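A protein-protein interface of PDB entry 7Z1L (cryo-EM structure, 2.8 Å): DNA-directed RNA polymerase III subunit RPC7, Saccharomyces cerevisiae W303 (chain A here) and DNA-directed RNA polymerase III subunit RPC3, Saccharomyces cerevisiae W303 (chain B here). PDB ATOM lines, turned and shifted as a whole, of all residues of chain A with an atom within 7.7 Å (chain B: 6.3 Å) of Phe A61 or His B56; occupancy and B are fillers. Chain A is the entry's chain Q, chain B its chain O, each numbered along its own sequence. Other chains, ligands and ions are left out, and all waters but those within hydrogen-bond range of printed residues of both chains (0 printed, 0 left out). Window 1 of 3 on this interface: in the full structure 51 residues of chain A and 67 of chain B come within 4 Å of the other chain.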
ATOM      1  N   ALA A  55     -28.144  22.868  24.154  1.00  0.00           N
ATOM      2  CA  ALA A  55     -27.127  22.004  23.563  1.00  0.00           C
ATOM      3  C   ALA A  55     -26.369  22.713  22.448  1.00  0.00           C
ATOM      4  O   ALA A  55     -25.147  22.555  22.326  1.00  0.00           O
ATOM      5  CB  ALA A  55     -27.767  20.720  23.038  1.00  0.00           C
ATOM      6  N   VAL A  56     -27.067  23.494  21.619  1.00  0.00           N
ATOM      7  CA  VAL A  56     -26.347  24.200  20.565  1.00  0.00           C
ATOM      8  C   VAL A  56     -25.525  25.339  21.162  1.00  0.00           C
ATOM      9  O   VAL A  56     -24.501  25.733  20.594  1.00  0.00           O
ATOM     10  CB  VAL A  56     -27.303  24.681  19.451  1.00  0.00           C
ATOM     11  CG1 VAL A  56     -28.227  25.771  19.933  1.00  0.00           C
ATOM     12  CG2 VAL A  56     -26.527  25.127  18.209  1.00  0.00           C
ATOM     13  N   LYS A  57     -25.921  25.859  22.330  1.00  0.00           N
ATOM     14  CA  LYS A  57     -25.059  26.804  23.038  1.00  0.00           C
ATOM     15  C   LYS A  57     -23.768  26.137  23.511  1.00  0.00           C
ATOM     16  O   LYS A  57     -22.680  26.709  23.359  1.00  0.00           O
ATOM     17  CB  LYS A  57     -25.814  27.426  24.211  1.00  0.00           C
ATOM     18  CG  LYS A  57     -26.719  28.578  23.801  1.00  0.00           C
ATOM     19  CD  LYS A  57     -27.375  29.233  25.000  1.00  0.00           C
ATOM     20  CE  LYS A  57     -28.124  30.490  24.592  1.00  0.00           C
ATOM     21  NZ  LYS A  57     -29.194  30.205  23.597  1.00  0.00           N
ATOM     22  N   TYR A  58     -23.872  24.931  24.088  1.00  0.00           N
ATOM     23  CA  TYR A  58     -22.679  24.120  24.359  1.00  0.00           C
ATOM     24  C   TYR A  58     -21.809  23.943  23.118  1.00  0.00           C
ATOM     25  O   TYR A  58     -20.584  24.111  23.179  1.00  0.00           O
ATOM     26  CB  TYR A  58     -23.058  22.743  24.913  1.00  0.00           C
ATOM     27  CG  TYR A  58     -23.638  22.675  26.308  1.00  0.00           C
ATOM     28  CD1 TYR A  58     -23.542  23.736  27.184  1.00  0.00           C
ATOM     29  CD2 TYR A  58     -24.266  21.525  26.751  1.00  0.00           C
ATOM     30  CE1 TYR A  58     -24.053  23.642  28.468  1.00  0.00           C
ATOM     31  CE2 TYR A  58     -24.779  21.425  28.017  1.00  0.00           C
ATOM     32  CZ  TYR A  58     -24.674  22.487  28.871  1.00  0.00           C
ATOM     33  OH  TYR A  58     -25.195  22.389  30.138  1.00  0.00           O
ATOM     34  N   ILE A  59     -22.423  23.577  21.991  1.00  0.00           N
ATOM     35  CA  ILE A  59     -21.652  23.286  20.783  1.00  0.00           C
ATOM     36  C   ILE A  59     -20.946  24.537  20.274  1.00  0.00           C
ATOM     37  O   ILE A  59     -19.767  24.495  19.898  1.00  0.00           O
ATOM     38  CB  ILE A  59     -22.561  22.665  19.705  1.00  0.00           C
ATOM     39  CG1 ILE A  59     -23.061  21.300  20.164  1.00  0.00           C
ATOM     40  CG2 ILE A  59     -21.821  22.523  18.388  1.00  0.00           C
ATOM     41  CD1 ILE A  59     -24.037  20.661  19.221  1.00  0.00           C
ATOM     42  N   ASN A  60     -21.651  25.672  20.264  1.00  0.00           N
ATOM     43  CA  ASN A  60     -21.051  26.920  19.804  1.00  0.00           C
ATOM     44  C   ASN A  60     -19.924  27.367  20.726  1.00  0.00           C
ATOM     45  O   ASN A  60     -18.891  27.858  20.255  1.00  0.00           O
ATOM     46  CB  ASN A  60     -22.119  28.004  19.688  1.00  0.00           C
ATOM     47  CG  ASN A  60     -22.933  27.883  18.418  1.00  0.00           C
ATOM     48  OD1 ASN A  60     -22.526  27.210  17.472  1.00  0.00           O
ATOM     49  ND2 ASN A  60     -24.089  28.532  18.389  1.00  0.00           N
ATOM     50  N   PHE A  61     -20.096  27.201  22.041  1.00  0.00           N
ATOM     51  CA  PHE A  61     -19.027  27.564  22.966  1.00  0.00           C
ATOM     52  C   PHE A  61     -17.800  26.679  22.775  1.00  0.00           C
ATOM     53  O   PHE A  61     -16.661  27.164  22.814  1.00  0.00           O
ATOM     54  CB  PHE A  61     -19.520  27.480  24.406  1.00  0.00           C
ATOM     55  CG  PHE A  61     -18.429  27.630  25.421  1.00  0.00           C
ATOM     56  CD1 PHE A  61     -17.854  28.865  25.652  1.00  0.00           C
ATOM     57  CD2 PHE A  61     -17.968  26.537  26.133  1.00  0.00           C
ATOM     58  CE1 PHE A  61     -16.848  29.009  26.576  1.00  0.00           C
ATOM     59  CE2 PHE A  61     -16.961  26.678  27.063  1.00  0.00           C
ATOM     60  CZ  PHE A  61     -16.402  27.915  27.287  1.00  0.00           C
ATOM     61  N   GLY A  62     -18.014  25.374  22.585  1.00  0.00           N
ATOM     62  CA  GLY A  62     -16.894  24.482  22.336  1.00  0.00           C
ATOM     63  C   GLY A  62     -16.166  24.809  21.048  1.00  0.00           C
ATOM     64  O   GLY A  62     -14.935  24.765  20.990  1.00  0.00           O
ATOM     65  N   LYS A  63     -16.919  25.153  20.000  1.00  0.00           N
ATOM     66  CA  LYS A  63     -16.301  25.558  18.741  1.00  0.00           C
ATOM     67  C   LYS A  63     -15.529  26.863  18.899  1.00  0.00           C
ATOM     68  O   LYS A  63     -14.468  27.042  18.290  1.00  0.00           O
ATOM     69  CB  LYS A  63     -17.366  25.688  17.655  1.00  0.00           C
ATOM     70  CG  LYS A  63     -16.852  25.449  16.248  1.00  0.00           C
ATOM     71  CD  LYS A  63     -17.971  25.006  15.322  1.00  0.00           C
ATOM     72  CE  LYS A  63     -19.052  26.068  15.216  1.00  0.00           C
ATOM     73  NZ  LYS A  63     -20.142  25.657  14.288  1.00  0.00           N
ATOM     74  N   THR A  64     -16.054  27.791  19.704  1.00  0.00           N
ATOM     75  CA  THR A  64     -15.369  29.060  19.935  1.00  0.00           C
ATOM     76  C   THR A  64     -14.051  28.851  20.672  1.00  0.00           C
ATOM     77  O   THR A  64     -13.023  29.431  20.305  1.00  0.00           O
ATOM     78  CB  THR A  64     -16.279  30.006  20.720  1.00  0.00           C
ATOM     79  OG1 THR A  64     -17.478  30.248  19.974  1.00  0.00           O
ATOM     80  CG2 THR A  64     -15.580  31.329  20.981  1.00  0.00           C
ATOM     81  N   VAL A  65     -14.065  28.021  21.717  1.00  0.00           N
ATOM     82  CA  VAL A  65     -12.844  27.780  22.485  1.00  0.00           C
ATOM     83  C   VAL A  65     -11.834  26.989  21.662  1.00  0.00           C
ATOM     84  O   VAL A  65     -10.625  27.243  21.729  1.00  0.00           O
ATOM     85  CB  VAL A  65     -13.179  27.076  23.813  1.00  0.00           C
ATOM     86  CG1 VAL A  65     -11.914  26.729  24.579  1.00  0.00           C
ATOM     87  CG2 VAL A  65     -14.055  27.964  24.654  1.00  0.00           C
ATOM     88  N   LYS A  66     -12.312  26.033  20.859  1.00  0.00           N
ATOM     89  CA  LYS A  66     -11.412  25.182  20.086  1.00  0.00           C
ATOM     90  C   LYS A  66     -10.624  25.986  19.056  1.00  0.00           C
ATOM     91  O   LYS A  66      -9.439  25.722  18.826  1.00  0.00           O
ATOM     92  CB  LYS A  66     -12.206  24.067  19.408  1.00  0.00           C
ATOM     93  CG  LYS A  66     -11.352  22.992  18.761  1.00  0.00           C
ATOM     94  CD  LYS A  66     -12.212  21.922  18.111  1.00  0.00           C
ATOM     95  CE  LYS A  66     -12.860  21.026  19.152  1.00  0.00           C
ATOM     96  NZ  LYS A  66     -11.858  20.183  19.857  1.00  0.00           N
ATOM     97  N   ASP A  67     -11.262  26.971  18.430  1.00  0.00           N
ATOM     98  CA  ASP A  67     -10.606  27.812  17.440  1.00  0.00           C
ATOM     99  C   ASP A  67     -10.037  29.097  18.029  1.00  0.00           C
ATOM    100  O   ASP A  67      -9.548  29.942  17.273  1.00  0.00           O
ATOM    101  CB  ASP A  67     -11.581  28.155  16.310  1.00  0.00           C
ATOM    102  CG  ASP A  67     -11.930  26.952  15.460  1.00  0.00           C
ATOM    103  OD1 ASP A  67     -11.084  26.040  15.344  1.00  0.00           O
ATOM    104  OD2 ASP A  67     -13.049  26.918  14.906  1.00  0.00           O
ATOM    105  N   GLY A  68     -10.086  29.266  19.349  1.00  0.00           N
ATOM    106  CA  GLY A  68      -9.598  30.471  19.973  1.00  0.00           C
ATOM    107  C   GLY A  68      -8.089  30.507  20.054  1.00  0.00           C
ATOM    108  O   GLY A  68      -7.378  29.598  19.602  1.00  0.00           O
ATOM    109  N   PHE A  70      -6.273  30.242  22.709  1.00  0.00           N
ATOM    110  CA  PHE A  70      -5.767  29.361  23.758  1.00  0.00           C
ATOM    111  C   PHE A  70      -6.269  27.949  23.471  1.00  0.00           C
ATOM    112  O   PHE A  70      -7.327  27.544  23.953  1.00  0.00           O
ATOM    113  CB  PHE A  70      -6.221  29.838  25.135  1.00  0.00           C
ATOM    114  CG  PHE A  70      -6.114  31.319  25.328  1.00  0.00           C
ATOM    115  CD1 PHE A  70      -4.877  31.929  25.433  1.00  0.00           C
ATOM    116  CD2 PHE A  70      -7.251  32.104  25.405  1.00  0.00           C
ATOM    117  CE1 PHE A  70      -4.776  33.294  25.612  1.00  0.00           C
ATOM    118  CE2 PHE A  70      -7.156  33.468  25.583  1.00  0.00           C
ATOM    119  CZ  PHE A  70      -5.916  34.063  25.684  1.00  0.00           C
ATOM    120  N   TYR A  71      -5.508  27.198  22.676  1.00  0.00           N
ATOM    121  CA  TYR A  71      -5.869  25.817  22.388  1.00  0.00           C
ATOM    122  C   TYR A  71      -4.809  24.822  22.829  1.00  0.00           C
ATOM    123  O   TYR A  71      -5.139  23.854  23.524  1.00  0.00           O
ATOM    124  CB  TYR A  71      -6.168  25.641  20.892  1.00  0.00           C
ATOM    125  CG  TYR A  71      -6.678  24.260  20.557  1.00  0.00           C
ATOM    126  CD1 TYR A  71      -7.922  23.837  20.999  1.00  0.00           C
ATOM    127  CD2 TYR A  71      -5.923  23.384  19.793  1.00  0.00           C
ATOM    128  CE1 TYR A  71      -8.395  22.575  20.701  1.00  0.00           C
ATOM    129  CE2 TYR A  71      -6.390  22.121  19.485  1.00  0.00           C
ATOM    130  CZ  TYR A  71      -7.626  21.723  19.943  1.00  0.00           C
ATOM    131  OH  TYR A  71      -8.093  20.465  19.638  1.00  0.00           O
ATOM    132  N   THR A  72      -3.543  25.044  22.463  1.00  0.00           N
ATOM    133  CA  THR A  72      -2.411  24.176  22.814  1.00  0.00           C
ATOM    134  C   THR A  72      -2.671  22.731  22.376  1.00  0.00           C
ATOM    135  O   THR A  72      -2.858  21.824  23.187  1.00  0.00           O
ATOM    136  CB  THR A  72      -2.076  24.246  24.310  1.00  0.00           C
ATOM    137  OG1 THR A  72      -3.190  23.797  25.091  1.00  0.00           O
ATOM    138  CG2 THR A  72      -1.723  25.670  24.709  1.00  0.00           C
ATOM    139  N   PHE A 153     -21.791  35.733  18.692  1.00  0.00           N
ATOM    140  CA  PHE A 153     -22.756  34.671  18.941  1.00  0.00           C
ATOM    141  C   PHE A 153     -23.724  34.543  17.771  1.00  0.00           C
ATOM    142  O   PHE A 153     -24.175  35.542  17.203  1.00  0.00           O
ATOM    143  CB  PHE A 153     -23.525  34.949  20.231  1.00  0.00           C
ATOM    144  CG  PHE A 153     -24.391  33.809  20.682  1.00  0.00           C
ATOM    145  CD1 PHE A 153     -23.831  32.683  21.261  1.00  0.00           C
ATOM    146  CD2 PHE A 153     -25.767  33.869  20.537  1.00  0.00           C
ATOM    147  CE1 PHE A 153     -24.627  31.634  21.682  1.00  0.00           C
ATOM    148  CE2 PHE A 153     -26.569  32.825  20.955  1.00  0.00           C
ATOM    149  CZ  PHE A 153     -25.998  31.705  21.528  1.00  0.00           C
ATOM    150  N   GLU B  51     -11.342  15.048  30.659  1.00  0.00           N
ATOM    151  CA  GLU B  51     -12.205  15.019  29.483  1.00  0.00           C
ATOM    152  C   GLU B  51     -12.680  16.414  29.103  1.00  0.00           C
ATOM    153  O   GLU B  51     -12.709  16.760  27.917  1.00  0.00           O
ATOM    154  CB  GLU B  51     -13.395  14.094  29.725  1.00  0.00           C
ATOM    155  CG  GLU B  51     -13.100  12.640  29.424  1.00  0.00           C
ATOM    156  CD  GLU B  51     -12.689  12.414  27.983  1.00  0.00           C
ATOM    157  OE1 GLU B  51     -13.354  12.964  27.080  1.00  0.00           O
ATOM    158  OE2 GLU B  51     -11.697  11.691  27.753  1.00  0.00           O
ATOM    159  N   LEU B  52     -13.046  17.235  30.091  1.00  0.00           N
ATOM    160  CA  LEU B  52     -13.494  18.595  29.796  1.00  0.00           C
ATOM    161  C   LEU B  52     -12.370  19.430  29.192  1.00  0.00           C
ATOM    162  O   LEU B  52     -12.574  20.143  28.199  1.00  0.00           O
ATOM    163  CB  LEU B  52     -14.031  19.256  31.064  1.00  0.00           C
ATOM    164  CG  LEU B  52     -15.476  18.930  31.430  1.00  0.00           C
ATOM    165  CD1 LEU B  52     -15.707  19.144  32.911  1.00  0.00           C
ATOM    166  CD2 LEU B  52     -16.433  19.775  30.611  1.00  0.00           C
ATOM    167  N   VAL B  53     -11.169  19.340  29.771  1.00  0.00           N
ATOM    168  CA  VAL B  53     -10.050  20.132  29.266  1.00  0.00           C
ATOM    169  C   VAL B  53      -9.634  19.650  27.880  1.00  0.00           C
ATOM    170  O   VAL B  53      -9.306  20.456  27.001  1.00  0.00           O
ATOM    171  CB  VAL B  53      -8.883  20.100  30.271  1.00  0.00           C
ATOM    172  CG1 VAL B  53      -7.651  20.748  29.688  1.00  0.00           C
ATOM    173  CG2 VAL B  53      -9.280  20.814  31.546  1.00  0.00           C
ATOM    174  N   LYS B  54      -9.671  18.335  27.646  1.00  0.00           N
ATOM    175  CA  LYS B  54      -9.328  17.805  26.331  1.00  0.00           C
ATOM    176  C   LYS B  54     -10.381  18.169  25.291  1.00  0.00           C
ATOM    177  O   LYS B  54     -10.061  18.345  24.111  1.00  0.00           O
ATOM    178  CB  LYS B  54      -9.154  16.290  26.408  1.00  0.00           C
ATOM    179  CG  LYS B  54      -8.304  15.703  25.299  1.00  0.00           C
ATOM    180  CD  LYS B  54      -8.259  14.187  25.390  1.00  0.00           C
ATOM    181  CE  LYS B  54      -9.527  13.566  24.833  1.00  0.00           C
ATOM    182  NZ  LYS B  54      -9.451  12.081  24.799  1.00  0.00           N
ATOM    183  N   ALA B  55     -11.646  18.267  25.705  1.00  0.00           N
ATOM    184  CA  ALA B  55     -12.697  18.655  24.772  1.00  0.00           C
ATOM    185  C   ALA B  55     -12.588  20.126  24.397  1.00  0.00           C
ATOM    186  O   ALA B  55     -12.752  20.486  23.226  1.00  0.00           O
ATOM    187  CB  ALA B  55     -14.069  18.354  25.373  1.00  0.00           C
ATOM    188  N   HIS B  56     -12.310  20.992  25.371  1.00  0.00           N
ATOM    189  CA  HIS B  56     -12.267  22.424  25.093  1.00  0.00           C
ATOM    190  C   HIS B  56     -10.877  22.878  24.652  1.00  0.00           C
ATOM    191  O   HIS B  56     -10.714  23.412  23.551  1.00  0.00           O
ATOM    192  CB  HIS B  56     -12.748  23.203  26.319  1.00  0.00           C
ATOM    193  CG  HIS B  56     -14.205  23.020  26.605  1.00  0.00           C
ATOM    194  ND1 HIS B  56     -14.725  21.840  27.092  1.00  0.00           N
ATOM    195  CD2 HIS B  56     -15.256  23.858  26.451  1.00  0.00           C
ATOM    196  CE1 HIS B  56     -16.032  21.964  27.237  1.00  0.00           C
ATOM    197  NE2 HIS B  56     -16.379  23.180  26.856  1.00  0.00           N
ATOM    198  N   LEU B  57      -9.869  22.671  25.494  1.00  0.00           N
ATOM    199  CA  LEU B  57      -8.497  22.960  25.113  1.00  0.00           C
ATOM    200  C   LEU B  57      -7.879  21.726  24.459  1.00  0.00           C
ATOM    201  O   LEU B  57      -8.563  20.752  24.139  1.00  0.00           O
ATOM    202  CB  LEU B  57      -7.689  23.422  26.324  1.00  0.00           C
ATOM    203  CG  LEU B  57      -8.330  24.525  27.169  1.00  0.00           C
ATOM    204  CD1 LEU B  57      -7.390  24.970  28.271  1.00  0.00           C
ATOM    205  CD2 LEU B  57      -8.721  25.705  26.303  1.00  0.00           C
ATOM    206  N   GLY B  58      -6.567  21.760  24.254  1.00  0.00           N
ATOM    207  CA  GLY B  58      -5.881  20.694  23.557  1.00  0.00           C
ATOM    208  C   GLY B  58      -5.500  19.542  24.466  1.00  0.00           C
ATOM    209  O   GLY B  58      -5.904  19.452  25.627  1.00  0.00           O
ATOM    210  N   LEU B 101      -7.795  30.992  31.189  1.00  0.00           N
ATOM    211  CA  LEU B 101      -9.155  30.494  31.353  1.00  0.00           C
ATOM    212  C   LEU B 101      -9.481  30.104  32.789  1.00  0.00           C
ATOM    213  O   LEU B 101     -10.493  29.429  33.008  1.00  0.00           O
ATOM    214  CB  LEU B 101      -9.410  29.298  30.430  1.00  0.00           C
ATOM    215  CG  LEU B 101      -9.757  29.571  28.963  1.00  0.00           C
ATOM    216  CD1 LEU B 101      -8.551  30.022  28.152  1.00  0.00           C
ATOM    217  CD2 LEU B 101     -10.401  28.347  28.336  1.00  0.00           C
ATOM    218  N   ILE B 129     -16.726  26.175  35.185  1.00  0.00           N
ATOM    219  CA  ILE B 129     -17.108  27.192  34.208  1.00  0.00           C
ATOM    220  C   ILE B 129     -17.194  26.575  32.817  1.00  0.00           C
ATOM    221  O   ILE B 129     -18.145  26.818  32.065  1.00  0.00           O
ATOM    222  CB  ILE B 129     -16.117  28.370  34.249  1.00  0.00           C
ATOM    223  CG1 ILE B 129     -16.386  29.257  35.466  1.00  0.00           C
ATOM    224  CG2 ILE B 129     -16.188  29.192  32.978  1.00  0.00           C
ATOM    225  CD1 ILE B 129     -17.737  29.912  35.455  1.00  0.00           C
ATOM    226  N   LEU B 130     -16.202  25.754  32.464  1.00  0.00           N
ATOM    227  CA  LEU B 130     -16.239  25.046  31.187  1.00  0.00           C
ATOM    228  C   LEU B 130     -17.393  24.052  31.126  1.00  0.00           C
ATOM    229  O   LEU B 130     -17.962  23.827  30.053  1.00  0.00           O
ATOM    230  CB  LEU B 130     -14.916  24.321  30.945  1.00  0.00           C
ATOM    231  CG  LEU B 130     -13.695  25.175  30.610  1.00  0.00           C
ATOM    232  CD1 LEU B 130     -12.541  24.291  30.170  1.00  0.00           C
ATOM    233  CD2 LEU B 130     -14.029  26.193  29.537  1.00  0.00           C
ATOM    234  N   LEU B 131     -17.744  23.449  32.260  1.00  0.00           N
ATOM    235  CA  LEU B 131     -18.813  22.459  32.302  1.00  0.00           C
ATOM    236  C   LEU B 131     -20.198  23.095  32.258  1.00  0.00           C
ATOM    237  O   LEU B 131     -21.126  22.512  31.685  1.00  0.00           O
ATOM    238  CB  LEU B 131     -18.657  21.602  33.559  1.00  0.00           C
ATOM    239  CG  LEU B 131     -19.742  20.607  33.961  1.00  0.00           C
ATOM    240  CD1 LEU B 131     -19.925  19.551  32.890  1.00  0.00           C
ATOM    241  CD2 LEU B 131     -19.380  19.968  35.289  1.00  0.00           C
ATOM    242  N   SER B 133     -21.107  26.064  30.879  1.00  0.00           N
ATOM    243  CA  SER B 133     -20.984  27.272  30.064  1.00  0.00           C
ATOM    244  C   SER B 133     -22.302  27.661  29.401  1.00  0.00           C
ATOM    245  O   SER B 133     -22.759  28.804  29.522  1.00  0.00           O
ATOM    246  CB  SER B 133     -19.896  27.075  29.013  1.00  0.00           C
ATOM    247  OG  SER B 133     -19.691  28.265  28.270  1.00  0.00           O
ATOM    248  N   GLY B 134     -22.927  26.723  28.688  1.00  0.00           N
ATOM    249  CA  GLY B 134     -24.199  27.028  28.052  1.00  0.00           C
ATOM    250  C   GLY B 134     -25.309  27.265  29.055  1.00  0.00           C
ATOM    251  O   GLY B 134     -26.192  28.097  28.833  1.00  0.00           O
ATOM    252  N   ILE B 137     -24.831  30.782  30.108  1.00  0.00           N
ATOM    253  CA  ILE B 137     -25.312  31.717  29.091  1.00  0.00           C
ATOM    254  C   ILE B 137     -26.834  31.802  29.113  1.00  0.00           C
ATOM    255  O   ILE B 137     -27.412  32.898  29.065  1.00  0.00           O
ATOM    256  CB  ILE B 137     -24.787  31.309  27.702  1.00  0.00           C
ATOM    257  CG1 ILE B 137     -23.264  31.435  27.650  1.00  0.00           C
ATOM    258  CG2 ILE B 137     -25.417  32.159  26.615  1.00  0.00           C
ATOM    259  CD1 ILE B 137     -22.649  30.879  26.387  1.00  0.00           C
ATOM    260  N   GLN B 161     -20.529  34.950  26.250  1.00  0.00           N
ATOM    261  CA  GLN B 161     -19.728  33.926  25.589  1.00  0.00           C
ATOM    262  C   GLN B 161     -18.277  34.367  25.444  1.00  0.00           C
ATOM    263  O   GLN B 161     -17.358  33.569  25.662  1.00  0.00           O
ATOM    264  CB  GLN B 161     -20.329  33.593  24.225  1.00  0.00           C
ATOM    265  CG  GLN B 161     -19.521  32.595  23.415  1.00  0.00           C
ATOM    266  CD  GLN B 161     -20.303  32.025  22.251  1.00  0.00           C
ATOM    267  OE1 GLN B 161     -21.136  31.137  22.422  1.00  0.00           O
ATOM    268  NE2 GLN B 161     -20.038  32.538  21.054  1.00  0.00           N
ATOM    269  N   ILE B 164     -16.572  34.170  28.933  1.00  0.00           N
ATOM    270  CA  ILE B 164     -16.265  32.804  29.351  1.00  0.00           C
ATOM    271  C   ILE B 164     -15.145  32.213  28.500  1.00  0.00           C
ATOM    272  O   ILE B 164     -14.249  31.534  29.016  1.00  0.00           O
ATOM    273  CB  ILE B 164     -17.532  31.931  29.311  1.00  0.00           C
ATOM    274  CG1 ILE B 164     -18.582  32.470  30.277  1.00  0.00           C
ATOM    275  CG2 ILE B 164     -17.212  30.509  29.706  1.00  0.00           C
ATOM    276  CD1 ILE B 164     -19.868  31.686  30.255  1.00  0.00           C
ATOM    277  N   SER B 165     -15.165  32.466  27.187  1.00  0.00           N
ATOM    278  CA  SER B 165     -14.159  31.884  26.303  1.00  0.00           C
ATOM    279  C   SER B 165     -12.785  32.498  26.535  1.00  0.00           C
ATOM    280  O   SER B 165     -11.768  31.802  26.440  1.00  0.00           O
ATOM    281  CB  SER B 165     -14.583  32.055  24.845  1.00  0.00           C
ATOM    282  OG  SER B 165     -14.575  33.420  24.469  1.00  0.00           O
ATOM    283  N   LYS B 592     -19.030  11.192  23.525  1.00  0.00           N
ATOM    284  CA  LYS B 592     -19.219  12.231  22.516  1.00  0.00           C
ATOM    285  C   LYS B 592     -17.912  12.561  21.808  1.00  0.00           C
ATOM    286  O   LYS B 592     -17.884  12.725  20.580  1.00  0.00           O
ATOM    287  CB  LYS B 592     -19.803  13.484  23.165  1.00  0.00           C
ATOM    288  CG  LYS B 592     -20.053  14.639  22.211  1.00  0.00           C
ATOM    289  CD  LYS B 592     -19.015  15.732  22.394  1.00  0.00           C
ATOM    290  CE  LYS B 592     -19.132  16.372  23.759  1.00  0.00           C
ATOM    291  NZ  LYS B 592     -18.159  17.484  23.925  1.00  0.00           N
ATOM    292  N   GLU B 593     -16.817  12.670  22.567  1.00  0.00           N
ATOM    293  CA  GLU B 593     -15.527  12.983  21.964  1.00  0.00           C
ATOM    294  C   GLU B 593     -15.055  11.861  21.048  1.00  0.00           C
ATOM    295  O   GLU B 593     -14.485  12.121  19.983  1.00  0.00           O
ATOM    296  CB  GLU B 593     -14.493  13.265  23.051  1.00  0.00           C
ATOM    297  CG  GLU B 593     -13.364  14.178  22.603  1.00  0.00           C
ATOM    298  CD  GLU B 593     -13.827  15.603  22.365  1.00  0.00           C
ATOM    299  OE1 GLU B 593     -14.780  16.042  23.044  1.00  0.00           O
ATOM    300  OE2 GLU B 593     -13.240  16.283  21.498  1.00  0.00           O
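The backbone carbonyl oxygen (O) of Ala B55 sits at hydrogen-bond distance from the side-chain amino group (NZ) of Lys A66 (3.5 Å).
N of Gly B58 is in hydrogen-bond range of O of Tyr A71, 2.6 Å away.
A ring nitrogen (ND1) of His B56 lies within hydrogen-bond range of the backbone carbonyl oxygen (O) of Leu B52 (3.0 Å).
OG of Ser B165 is in hydrogen-bond range of O of Gln B161 (3.0 Å).
O of Asn A60 sits at hydrogen-bond distance from OG1 of Thr A64, at 2.8 Å.
Among the printed residues, merely in contact across the chains: Lys A57 with Ile B137, Tyr A58 with Gly B134, Phe A61 with His B56, Phe A61 with Leu B130, Phe A61 with Ser B133, Phe A61 with Ile B164, Phe A61 with Ser B165, Thr A64 with Gln B161, Val A65 with His B56, Val A65 with Leu B57, Lys A66 with His B56, Phe A70 with Leu B57, Phe A70 with Leu B101, Tyr A71 with His B56, Tyr A71 with Leu B57, Thr A72 with Gly B58 and Phe A153 with Gln B161.
Lys A63 touches none of the printed residues of chain B.
Printed residues of chain B within 4 Å of Phe A70: Leu B57 (3.3 Å) and Leu B101 (3.7 Å).
Lys B54 touches none of the printed residues of chain A.
Of the printed residues of chain A, Leu B130 touches Phe A61 (3.7 Å).
Printed residues of chain A within 4 Å of Ser B133: Phe A61.
Printed residues of chain A within 4 Å of Gly B134: Tyr A58 (3.3 Å).
Of the printed residues of chain A, Ile B164 touches Phe A61.
The nearest residue of chain B that does not touch Phe A61 is Gln B161 (4.1 Å).
The nearest residue of chain A that does not touch His B56 is Gly A62 (4.5 Å).
Of the 18 printed residues of chain A, 10 touch a printed residue of chain B.
Printed residues of chain A that touch a printed residue of chain B: Lys A57, Tyr A58, Phe A61, Thr A64, Val A65, Lys A66, Phe A70, Tyr A71, Thr A72 and Phe A153.
Hydrophobic or aromatic side chains of chain A that line the printed part of chain B: Tyr A58, Phe A61, Val A65, Phe A70, Tyr A71 and Phe A153.
Of the 20 printed residues of chain B, 12 touch a printed residue of chain A.
Printed residues of chain B that touch a printed residue of chain A: Ala B55, His B56, Leu B57, Gly B58, Leu B101, Leu B130, Ser B133, Gly B134, Ile B137, Gln B161, Ile B164 and Ser B165.
Hydrophobic or aromatic side chains of chain B that line the printed part of chain A: His B56, Leu B57, Leu B101, Leu B130, Ile B137 and Ile B164.
Among the printed residues, no Asp or Glu carboxylate lies within 4 Å of a Lys or Arg side-chain nitrogen of the other chain.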
